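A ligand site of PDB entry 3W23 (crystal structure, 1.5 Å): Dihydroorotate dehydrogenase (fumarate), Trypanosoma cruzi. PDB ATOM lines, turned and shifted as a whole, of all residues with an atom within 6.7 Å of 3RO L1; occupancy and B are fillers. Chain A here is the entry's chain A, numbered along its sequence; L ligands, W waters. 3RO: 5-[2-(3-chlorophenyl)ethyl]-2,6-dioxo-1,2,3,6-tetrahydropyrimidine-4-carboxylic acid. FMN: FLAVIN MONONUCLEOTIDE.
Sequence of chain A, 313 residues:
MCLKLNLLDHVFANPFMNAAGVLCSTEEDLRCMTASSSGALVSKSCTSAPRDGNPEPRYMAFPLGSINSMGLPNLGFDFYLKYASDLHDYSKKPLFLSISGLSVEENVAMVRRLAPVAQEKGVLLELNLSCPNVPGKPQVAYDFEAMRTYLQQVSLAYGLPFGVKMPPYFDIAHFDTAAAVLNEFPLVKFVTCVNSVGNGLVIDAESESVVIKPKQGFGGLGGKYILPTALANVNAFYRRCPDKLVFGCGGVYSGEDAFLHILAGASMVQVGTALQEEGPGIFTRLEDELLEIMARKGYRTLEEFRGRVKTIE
Water W1 bridges OAA of 3RO L1 (2.9 Å) and O of Asn 68 (3.1 Å). Water W2 lies within hydrogen-bond range of the backbone NH (N) of Gly 71 (3.1 Å), an oxygen (OAA) of 3RO L1 (3.2 Å) and the side-chain amide nitrogen (ND2) of Asn 54 (3.4 Å).
OAB of 3RO L1 lies within hydrogen-bond range of OG of Ser 196, 2.8 Å away. A nitrogen (NAM) of 3RO L1 lies within hydrogen-bond range of the side-chain amide oxygen (OD1) of Asn 195 (2.8 Å). N of Leu 72 lies within hydrogen-bond range of OAD of 3RO L1 (2.9 Å). OAB of 3RO L1 sits at hydrogen-bond distance from ND2 of Asn 68 (2.9 Å). The side-chain amide nitrogen (ND2) of Asn 128 sits at hydrogen-bond distance from an oxygen (OAC) of 3RO L1. The backbone NH (N) of Met 70 lies within hydrogen-bond range of an oxygen (OAA) of 3RO L1, at 3.1 Å. The backbone NH (N) of Gly 71 sits at hydrogen-bond distance from an oxygen (OAA) of 3RO L1, 3.2 Å away. NZ of Lys 44 lies within salt-bridge range of OAD of 3RO L1. ND2 of Asn 195 is in hydrogen-bond range of O2 of FMN L2. The side-chain amide nitrogen (ND2) of Asn 128 sits at hydrogen-bond distance from an oxygen (O2) of FMN L2, 3.5 Å away. NZ of Lys 44 is in hydrogen-bond range of O4 of FMN L2, at 2.7 Å. N3 of FMN L2 is in hydrogen-bond range of OG of Ser 45 (2.8 Å). The side-chain amino group (NZ) of Lys 165 is in hydrogen-bond range of an oxygen (O2') of FMN L2 (2.8 Å). The backbone carbonyl oxygen of Ala 20 is in hydrogen-bond range of an oxygen (O2') of FMN L2, at 2.8 Å.
NAM of 3RO L1 sits close to N1 of FMN L2 (3.5 Å).
OD1 of Asn 195 lies within hydrogen-bond range of OG of Ser 196 (3.5 Å). O of Leu 72 is in hydrogen-bond range of NE of Arg 51, 3.3 Å away. OD1 of Asn 68 is in hydrogen-bond range of N of Met 70 (3.3 Å). The backbone carbonyl oxygen of Asn 68 lies within hydrogen-bond range of the backbone NH of Gly 220, 2.8 Å away. The backbone NH of Ser 130 is in hydrogen-bond range of the side-chain amide oxygen of Asn 128. OG of Ser 100 is in hydrogen-bond range of ND2 of Asn 128 (3.3 Å). The backbone NH (N) of Asn 54 sits at hydrogen-bond distance from the backbone carbonyl oxygen (O) of Met 70 (2.8 Å). O of Ser 69 lies within hydrogen-bond range of ND2 of Asn 54, 2.9 Å away.
Arg 51 touches 3RO L1. C of Ser 69 touches OAA of 3RO L1, 3.9 Å away. Ser 130 touches 3RO L1 (O to OAC, 3.5 Å). CD of Pro 132 touches CAI of 3RO L1, 3.5 Å away. Hydrophobic or aromatic side chains that line 3RO L1: Met 70, Leu 72 and Pro 132. Within 4 Å of 3RO L1: Lys 44, Arg 51, Asn 68, Ser 69, Met 70, Gly 71, Leu 72, Asn 128, Ser 130, Pro 132, Asn 195 and Ser 196.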
ATOM      1  N   ALA A  20      10.918 -31.322 -10.079  1.00  0.00           N
ATOM      2  CA  ALA A  20      12.094 -32.060 -10.505  1.00  0.00           C
ATOM      3  C   ALA A  20      13.064 -32.231  -9.331  1.00  0.00           C
ATOM      4  O   ALA A  20      13.311 -31.308  -8.574  1.00  0.00           O
ATOM      5  CB  ALA A  20      12.772 -31.381 -11.689  1.00  0.00           C
ATOM      6  N   LYS A  44      13.911 -36.687 -12.848  1.00  0.00           N
ATOM      7  CA  LYS A  44      15.089 -36.019 -12.311  1.00  0.00           C
ATOM      8  C   LYS A  44      15.909 -35.336 -13.425  1.00  0.00           C
ATOM      9  O   LYS A  44      16.228 -36.031 -14.396  1.00  0.00           O
ATOM     10  CB  LYS A  44      15.977 -37.046 -11.585  1.00  0.00           C
ATOM     11  CG  LYS A  44      17.285 -36.494 -11.078  1.00  0.00           C
ATOM     12  CD  LYS A  44      17.263 -35.370  -9.955  1.00  0.00           C
ATOM     13  CE  LYS A  44      18.593 -34.587  -9.772  1.00  0.00           C
ATOM     14  NZ  LYS A  44      18.719 -33.474  -8.692  1.00  0.00           N
ATOM     15  N   SER A  45      16.317 -34.097 -13.167  1.00  0.00           N
ATOM     16  CA  SER A  45      17.180 -33.381 -14.177  1.00  0.00           C
ATOM     17  C   SER A  45      18.391 -34.262 -14.395  1.00  0.00           C
ATOM     18  O   SER A  45      18.996 -34.778 -13.503  1.00  0.00           O
ATOM     19  CB  SER A  45      17.676 -32.063 -13.675  1.00  0.00           C
ATOM     20  OG  SER A  45      16.557 -31.202 -13.562  1.00  0.00           O
ATOM     21  N   ARG A  51      25.719 -39.414 -12.765  1.00  0.00           N
ATOM     22  CA  ARG A  51      26.441 -38.691 -11.726  1.00  0.00           C
ATOM     23  C   ARG A  51      26.083 -39.237 -10.353  1.00  0.00           C
ATOM     24  O   ARG A  51      24.963 -39.461 -10.094  1.00  0.00           O
ATOM     25  CB  ARG A  51      26.066 -37.212 -11.703  1.00  0.00           C
ATOM     26  CG  ARG A  51      26.546 -36.434 -12.888  1.00  0.00           C
ATOM     27  CD  ARG A  51      26.105 -34.972 -12.882  1.00  0.00           C
ATOM     28  NE  ARG A  51      26.467 -34.224 -11.695  1.00  0.00           N
ATOM     29  CZ  ARG A  51      27.580 -33.539 -11.579  1.00  0.00           C
ATOM     30  NH1 ARG A  51      28.462 -33.548 -12.536  1.00  0.00           N
ATOM     31  NH2 ARG A  51      27.834 -32.879 -10.492  1.00  0.00           N
ATOM     32  N   ASN A  54      26.994 -34.927  -4.957  1.00  0.00           N
ATOM     33  CA  ASN A  54      27.815 -34.500  -3.879  1.00  0.00           C
ATOM     34  C   ASN A  54      27.791 -35.442  -2.666  1.00  0.00           C
ATOM     35  O   ASN A  54      26.946 -36.222  -2.480  1.00  0.00           O
ATOM     36  CB  ASN A  54      27.392 -33.086  -3.422  1.00  0.00           C
ATOM     37  CG  ASN A  54      27.767 -32.006  -4.376  1.00  0.00           C
ATOM     38  OD1 ASN A  54      28.633 -32.138  -5.193  1.00  0.00           O
ATOM     39  ND2 ASN A  54      27.063 -30.916  -4.291  1.00  0.00           N
ATOM     40  N   ASN A  68      19.429 -27.858   0.143  1.00  0.00           N
ATOM     41  CA  ASN A  68      20.071 -28.953  -0.605  1.00  0.00           C
ATOM     42  C   ASN A  68      21.243 -28.431  -1.416  1.00  0.00           C
ATOM     43  O   ASN A  68      21.196 -27.387  -2.028  1.00  0.00           O
ATOM     44  CB  ASN A  68      19.108 -29.776  -1.497  1.00  0.00           C
ATOM     45  CG  ASN A  68      18.903 -29.173  -2.843  1.00  0.00           C
ATOM     46  OD1 ASN A  68      19.719 -29.404  -3.751  1.00  0.00           O
ATOM     47  ND2 ASN A  68      17.861 -28.414  -3.012  1.00  0.00           N
ATOM     48  N   SER A  69      22.278 -29.227  -1.530  1.00  0.00           N
ATOM     49  CA  SER A  69      23.307 -29.117  -2.558  1.00  0.00           C
ATOM     50  C   SER A  69      23.555 -30.522  -3.033  1.00  0.00           C
ATOM     51  O   SER A  69      24.589 -31.114  -2.755  1.00  0.00           O
ATOM     52  CB  SER A  69      24.522 -28.451  -1.953  1.00  0.00           C
ATOM     53  OG  SER A  69      24.294 -27.068  -1.720  1.00  0.00           O
ATOM     54  N   MET A  70      22.601 -31.097  -3.787  1.00  0.00           N
ATOM     55  CA  MET A  70      22.658 -32.473  -4.201  1.00  0.00           C
ATOM     56  C   MET A  70      23.815 -32.733  -5.179  1.00  0.00           C
ATOM     57  O   MET A  70      24.439 -33.783  -5.181  1.00  0.00           O
ATOM     58  CB  MET A  70      21.382 -32.840  -4.898  1.00  0.00           C
ATOM     59  CG  MET A  70      20.127 -32.740  -4.080  1.00  0.00           C
ATOM     60  SD  MET A  70      20.101 -33.628  -2.555  1.00  0.00           S
ATOM     61  CE  MET A  70      20.036 -35.286  -3.115  1.00  0.00           C
ATOM     62  N   GLY A  71      24.113 -31.777  -6.053  1.00  0.00           N
ATOM     63  CA  GLY A  71      25.152 -31.907  -7.092  1.00  0.00           C
ATOM     64  C   GLY A  71      24.714 -32.705  -8.241  1.00  0.00           C
ATOM     65  O   GLY A  71      25.486 -33.403  -8.898  1.00  0.00           O
ATOM     66  N   LEU A  72      23.447 -32.673  -8.543  1.00  0.00           N
ATOM     67  CA  LEU A  72      22.840 -33.269  -9.700  1.00  0.00           C
ATOM     68  C   LEU A  72      23.110 -34.799  -9.788  1.00  0.00           C
ATOM     69  O   LEU A  72      23.453 -35.342 -10.879  1.00  0.00           O
ATOM     70  CB  LEU A  72      23.198 -32.491 -10.976  1.00  0.00           C
ATOM     71  CG  LEU A  72      22.482 -32.601 -12.325  1.00  0.00           C
ATOM     72  CD1 LEU A  72      21.030 -32.513 -12.084  1.00  0.00           C
ATOM     73  CD2 LEU A  72      22.986 -31.467 -13.208  1.00  0.00           C
ATOM     74  N   PRO A  73      22.930 -35.546  -8.755  1.00  0.00           N
ATOM     75  CA  PRO A  73      22.941 -37.025  -8.863  1.00  0.00           C
ATOM     76  C   PRO A  73      21.849 -37.489  -9.813  1.00  0.00           C
ATOM     77  O   PRO A  73      20.728 -37.052  -9.748  1.00  0.00           O
ATOM     78  CB  PRO A  73      22.730 -37.526  -7.491  1.00  0.00           C
ATOM     79  CG  PRO A  73      21.909 -36.482  -6.783  1.00  0.00           C
ATOM     80  CD  PRO A  73      22.285 -35.144  -7.465  1.00  0.00           C
ATOM     81  N   SER A 100      19.421 -31.079 -17.565  1.00  0.00           N
ATOM     82  CA  SER A 100      20.193 -30.006 -16.984  1.00  0.00           C
ATOM     83  C   SER A 100      21.662 -30.245 -17.293  1.00  0.00           C
ATOM     84  O   SER A 100      22.519 -30.447 -16.424  1.00  0.00           O
ATOM     85  CB  SER A 100      19.876 -30.000 -15.478  1.00  0.00           C
ATOM     86  OG  SER A 100      20.520 -28.942 -14.784  1.00  0.00           O
ATOM     87  N   LEU A 102      25.519 -29.495 -18.333  1.00  0.00           N
ATOM     88  CA  LEU A 102      26.469 -28.632 -17.702  1.00  0.00           C
ATOM     89  C   LEU A 102      27.152 -27.641 -18.661  1.00  0.00           C
ATOM     90  O   LEU A 102      27.972 -26.802 -18.235  1.00  0.00           O
ATOM     91  CB  LEU A 102      27.442 -29.424 -16.814  1.00  0.00           C
ATOM     92  CG  LEU A 102      26.651 -30.037 -15.545  1.00  0.00           C
ATOM     93  CD1 LEU A 102      27.471 -30.948 -14.699  1.00  0.00           C
ATOM     94  CD2 LEU A 102      26.149 -28.973 -14.557  1.00  0.00           C
ATOM     95  N   ASN A 128      16.213 -27.179 -17.476  1.00  0.00           N
ATOM     96  CA  ASN A 128      16.632 -26.479 -16.271  1.00  0.00           C
ATOM     97  C   ASN A 128      17.641 -25.448 -16.555  1.00  0.00           C
ATOM     98  O   ASN A 128      18.763 -25.776 -16.887  1.00  0.00           O
ATOM     99  CB  ASN A 128      17.110 -27.485 -15.245  1.00  0.00           C
ATOM    100  CG  ASN A 128      17.462 -26.845 -13.945  1.00  0.00           C
ATOM    101  OD1 ASN A 128      17.049 -25.773 -13.621  1.00  0.00           O
ATOM    102  ND2 ASN A 128      17.997 -27.676 -13.096  1.00  0.00           N
ATOM    103  N   SER A 130      18.305 -23.035 -14.120  1.00  0.00           N
ATOM    104  CA  SER A 130      18.880 -22.680 -12.816  1.00  0.00           C
ATOM    105  C   SER A 130      19.893 -23.712 -12.529  1.00  0.00           C
ATOM    106  O   SER A 130      19.683 -24.606 -11.787  1.00  0.00           O
ATOM    107  CB  SER A 130      17.865 -22.621 -11.715  1.00  0.00           C
ATOM    108  OG  SER A 130      18.436 -22.408 -10.463  1.00  0.00           O
ATOM    109  N   CYS A 131      21.006 -23.590 -13.215  1.00  0.00           N
ATOM    110  CA  CYS A 131      21.991 -24.559 -13.350  1.00  0.00           C
ATOM    111  C   CYS A 131      23.407 -23.889 -13.571  1.00  0.00           C
ATOM    112  O   CYS A 131      23.547 -22.947 -14.273  1.00  0.00           O
ATOM    113  CB  CYS A 131      21.668 -25.323 -14.639  1.00  0.00           C
ATOM    114  SG  CYS A 131      22.665 -26.798 -14.925  1.00  0.00           S
ATOM    115  N   PRO A 132      24.472 -24.584 -12.984  1.00  0.00           N
ATOM    116  CA  PRO A 132      25.818 -24.049 -13.302  1.00  0.00           C
ATOM    117  C   PRO A 132      26.234 -24.089 -14.764  1.00  0.00           C
ATOM    118  O   PRO A 132      25.838 -24.906 -15.483  1.00  0.00           O
ATOM    119  CB  PRO A 132      26.778 -24.975 -12.521  1.00  0.00           C
ATOM    120  CG  PRO A 132      26.000 -25.569 -11.451  1.00  0.00           C
ATOM    121  CD  PRO A 132      24.667 -25.812 -12.043  1.00  0.00           C
ATOM    122  N   LYS A 165      12.693 -24.285 -16.620  1.00  0.00           N
ATOM    123  CA  LYS A 165      12.662 -24.167 -15.164  1.00  0.00           C
ATOM    124  C   LYS A 165      13.564 -23.011 -14.809  1.00  0.00           C
ATOM    125  O   LYS A 165      14.778 -23.008 -15.141  1.00  0.00           O
ATOM    126  CB  LYS A 165      13.175 -25.427 -14.518  1.00  0.00           C
ATOM    127  CG  LYS A 165      13.247 -25.438 -12.986  1.00  0.00           C
ATOM    128  CD  LYS A 165      11.891 -25.535 -12.321  1.00  0.00           C
ATOM    129  CE  LYS A 165      11.977 -25.852 -10.871  1.00  0.00           C
ATOM    130  NZ  LYS A 165      12.413 -27.203 -10.563  1.00  0.00           N
ATOM    131  N   ASN A 195      12.756 -22.581  -9.202  1.00  0.00           N
ATOM    132  CA  ASN A 195      13.774 -23.425  -8.594  1.00  0.00           C
ATOM    133  C   ASN A 195      14.065 -22.877  -7.171  1.00  0.00           C
ATOM    134  O   ASN A 195      13.509 -21.933  -6.792  1.00  0.00           O
ATOM    135  CB  ASN A 195      15.043 -23.512  -9.490  1.00  0.00           C
ATOM    136  CG  ASN A 195      15.742 -24.874  -9.424  1.00  0.00           C
ATOM    137  OD1 ASN A 195      15.981 -25.357  -8.382  1.00  0.00           O
ATOM    138  ND2 ASN A 195      15.982 -25.457 -10.558  1.00  0.00           N
ATOM    139  N   SER A 196      14.923 -23.568  -6.452  1.00  0.00           N
ATOM    140  CA  SER A 196      15.224 -23.175  -5.103  1.00  0.00           C
ATOM    141  C   SER A 196      15.846 -21.781  -4.998  1.00  0.00           C
ATOM    142  O   SER A 196      16.397 -21.304  -5.894  1.00  0.00           O
ATOM    143  CB  SER A 196      16.119 -24.243  -4.435  1.00  0.00           C
ATOM    144  OG  SER A 196      17.143 -24.621  -5.208  1.00  0.00           O
ATOM    145  N   LYS A 215      29.798 -27.317  -0.165  1.00  0.00           N
ATOM    146  CA  LYS A 215      29.748 -25.874  -0.296  1.00  0.00           C
ATOM    147  C   LYS A 215      29.717 -25.182   1.055  1.00  0.00           C
ATOM    148  O   LYS A 215      29.111 -24.106   1.234  1.00  0.00           O
ATOM    149  CB  LYS A 215      28.549 -25.450  -1.155  1.00  0.00           C
ATOM    150  CG  LYS A 215      28.650 -25.928  -2.585  1.00  0.00           C
ATOM    151  CD  LYS A 215      27.394 -25.474  -3.363  1.00  0.00           C
ATOM    152  CE  LYS A 215      26.999 -24.012  -3.254  1.00  0.00           C
ATOM    153  NZ  LYS A 215      25.995 -23.657  -4.302  1.00  0.00           N
ATOM    154  N   GLY A 220      20.513 -24.632  -1.833  1.00  0.00           N
ATOM    155  CA  GLY A 220      19.256 -24.018  -2.282  1.00  0.00           C
ATOM    156  C   GLY A 220      18.124 -24.286  -1.307  1.00  0.00           C
ATOM    157  O   GLY A 220      17.978 -25.377  -0.770  1.00  0.00           O
ATOM    158  N   LEU A 221      17.287 -23.277  -1.052  1.00  0.00           N
ATOM    159  CA  LEU A 221      16.157 -23.341  -0.116  1.00  0.00           C
ATOM    160  C   LEU A 221      14.857 -23.642  -0.797  1.00  0.00           C
ATOM    161  O   LEU A 221      14.586 -23.071  -1.856  1.00  0.00           O
ATOM    162  CB  LEU A 221      16.018 -21.998   0.599  1.00  0.00           C
ATOM    163  CG  LEU A 221      17.264 -21.462   1.336  1.00  0.00           C
ATOM    164  CD1 LEU A 221      17.085 -20.060   1.821  1.00  0.00           C
ATOM    165  CD2 LEU A 221      17.611 -22.332   2.486  1.00  0.00           C
HETATM  166  OAA 3RO L   1      21.789 -29.674  -6.425  1.00  0.00           O
HETATM  167  CAN 3RO L   1      21.115 -30.159  -7.342  1.00  0.00           C
HETATM  168  OAD 3RO L   1      21.067 -31.237  -7.909  1.00  0.00           O
HETATM  169  CAQ 3RO L   1      19.927 -29.211  -7.684  1.00  0.00           C
HETATM  170  NAL 3RO L   1      19.176 -28.749  -6.564  1.00  0.00           N
HETATM  171  CAS 3RO L   1      18.164 -27.796  -6.675  1.00  0.00           C
HETATM  172  OAB 3RO L   1      17.549 -27.347  -5.691  1.00  0.00           O
HETATM  173  NAM 3RO L   1      17.872 -27.405  -7.942  1.00  0.00           N
HETATM  174  CAT 3RO L   1      18.522 -27.846  -9.112  1.00  0.00           C
HETATM  175  OAC 3RO L   1      18.151 -27.384 -10.210  1.00  0.00           O
HETATM  176  CAR 3RO L   1      19.568 -28.793  -8.932  1.00  0.00           C
HETATM  177  CAK 3RO L   1      20.260 -29.194 -10.119  1.00  0.00           C
HETATM  178  CAJ 3RO L   1      21.290 -28.075 -10.707  1.00  0.00           C
HETATM  179  CAP 3RO L   1      22.437 -28.011 -10.050  1.00  0.00           C
HETATM  180  CAI 3RO L   1      23.542 -28.782 -10.494  1.00  0.00           C
HETATM  181  CAO 3RO L   1      24.690 -28.642  -9.701  1.00  0.00           C
HETATM  182 CL1  3RO L   1      26.088 -29.665 -10.151  1.00  0.00          CL
HETATM  183  CAG 3RO L   1      24.798 -27.816  -8.568  1.00  0.00           C
HETATM  184  CAF 3RO L   1      23.736 -27.025  -8.204  1.00  0.00           C
HETATM  185  CAH 3RO L   1      22.548 -27.086  -8.972  1.00  0.00           C
HETATM  186  N1  FMN L   2      15.047 -28.597  -9.568  1.00  0.00           N
HETATM  187  C2  FMN L   2      15.392 -29.000 -10.840  1.00  0.00           C
HETATM  188  O2  FMN L   2      14.844 -28.352 -11.755  1.00  0.00           O
HETATM  189  N3  FMN L   2      16.099 -30.092 -11.075  1.00  0.00           N
HETATM  190  C4  FMN L   2      16.555 -30.884 -10.115  1.00  0.00           C
HETATM  191  O4  FMN L   2      17.193 -31.936 -10.366  1.00  0.00           O
HETATM  192  C4A FMN L   2      16.323 -30.496  -8.778  1.00  0.00           C
HETATM  193  N5  FMN L   2      16.725 -31.277  -7.757  1.00  0.00           N
HETATM  194  C5A FMN L   2      16.206 -31.103  -6.492  1.00  0.00           C
HETATM  195  C6  FMN L   2      16.529 -31.982  -5.462  1.00  0.00           C
HETATM  196  C7  FMN L   2      16.065 -31.749  -4.178  1.00  0.00           C
HETATM  197  C7M FMN L   2      16.406 -32.729  -3.050  1.00  0.00           C
HETATM  198  C8  FMN L   2      15.251 -30.631  -3.929  1.00  0.00           C
HETATM  199  C8M FMN L   2      14.715 -30.342  -2.548  1.00  0.00           C
HETATM  200  C9  FMN L   2      14.956 -29.713  -4.918  1.00  0.00           C
HETATM  201  C9A FMN L   2      15.414 -29.937  -6.188  1.00  0.00           C
HETATM  202  N10 FMN L   2      15.113 -29.042  -7.262  1.00  0.00           N
HETATM  203  C10 FMN L   2      15.471 -29.375  -8.570  1.00  0.00           C
HETATM  204  C1' FMN L   2      14.274 -27.870  -6.976  1.00  0.00           C
HETATM  205  C2' FMN L   2      12.821 -28.201  -6.890  1.00  0.00           C
HETATM  206  O2' FMN L   2      12.372 -28.714  -8.168  1.00  0.00           O
HETATM  207  C3' FMN L   2      11.967 -27.028  -6.561  1.00  0.00           C
HETATM  208  O3' FMN L   2      12.116 -26.062  -7.624  1.00  0.00           O
HETATM  209  C4' FMN L   2      12.386 -26.347  -5.243  1.00  0.00           C
HETATM  210  O4' FMN L   2      12.638 -27.410  -4.268  1.00  0.00           O
HETATM  211  C5' FMN L   2      11.281 -25.450  -4.705  1.00  0.00           C
HETATM  212  O5' FMN L   2      10.037 -26.128  -4.508  1.00  0.00           O
HETATM  213  P   FMN L   2       9.530 -26.550  -3.005  1.00  0.00           P
HETATM  214  O1P FMN L   2       8.233 -27.323  -3.225  1.00  0.00           O
HETATM  215  O2P FMN L   2       9.446 -25.272  -2.187  1.00  0.00           O
HETATM  216  O3P FMN L   2      10.670 -27.446  -2.440  1.00  0.00           O
HETATM  217  O   HOH W   1      21.532 -27.065  -5.074  1.00  0.00           O
HETATM  218  O   HOH W   2      24.699 -28.747  -5.502  1.00  0.00           O
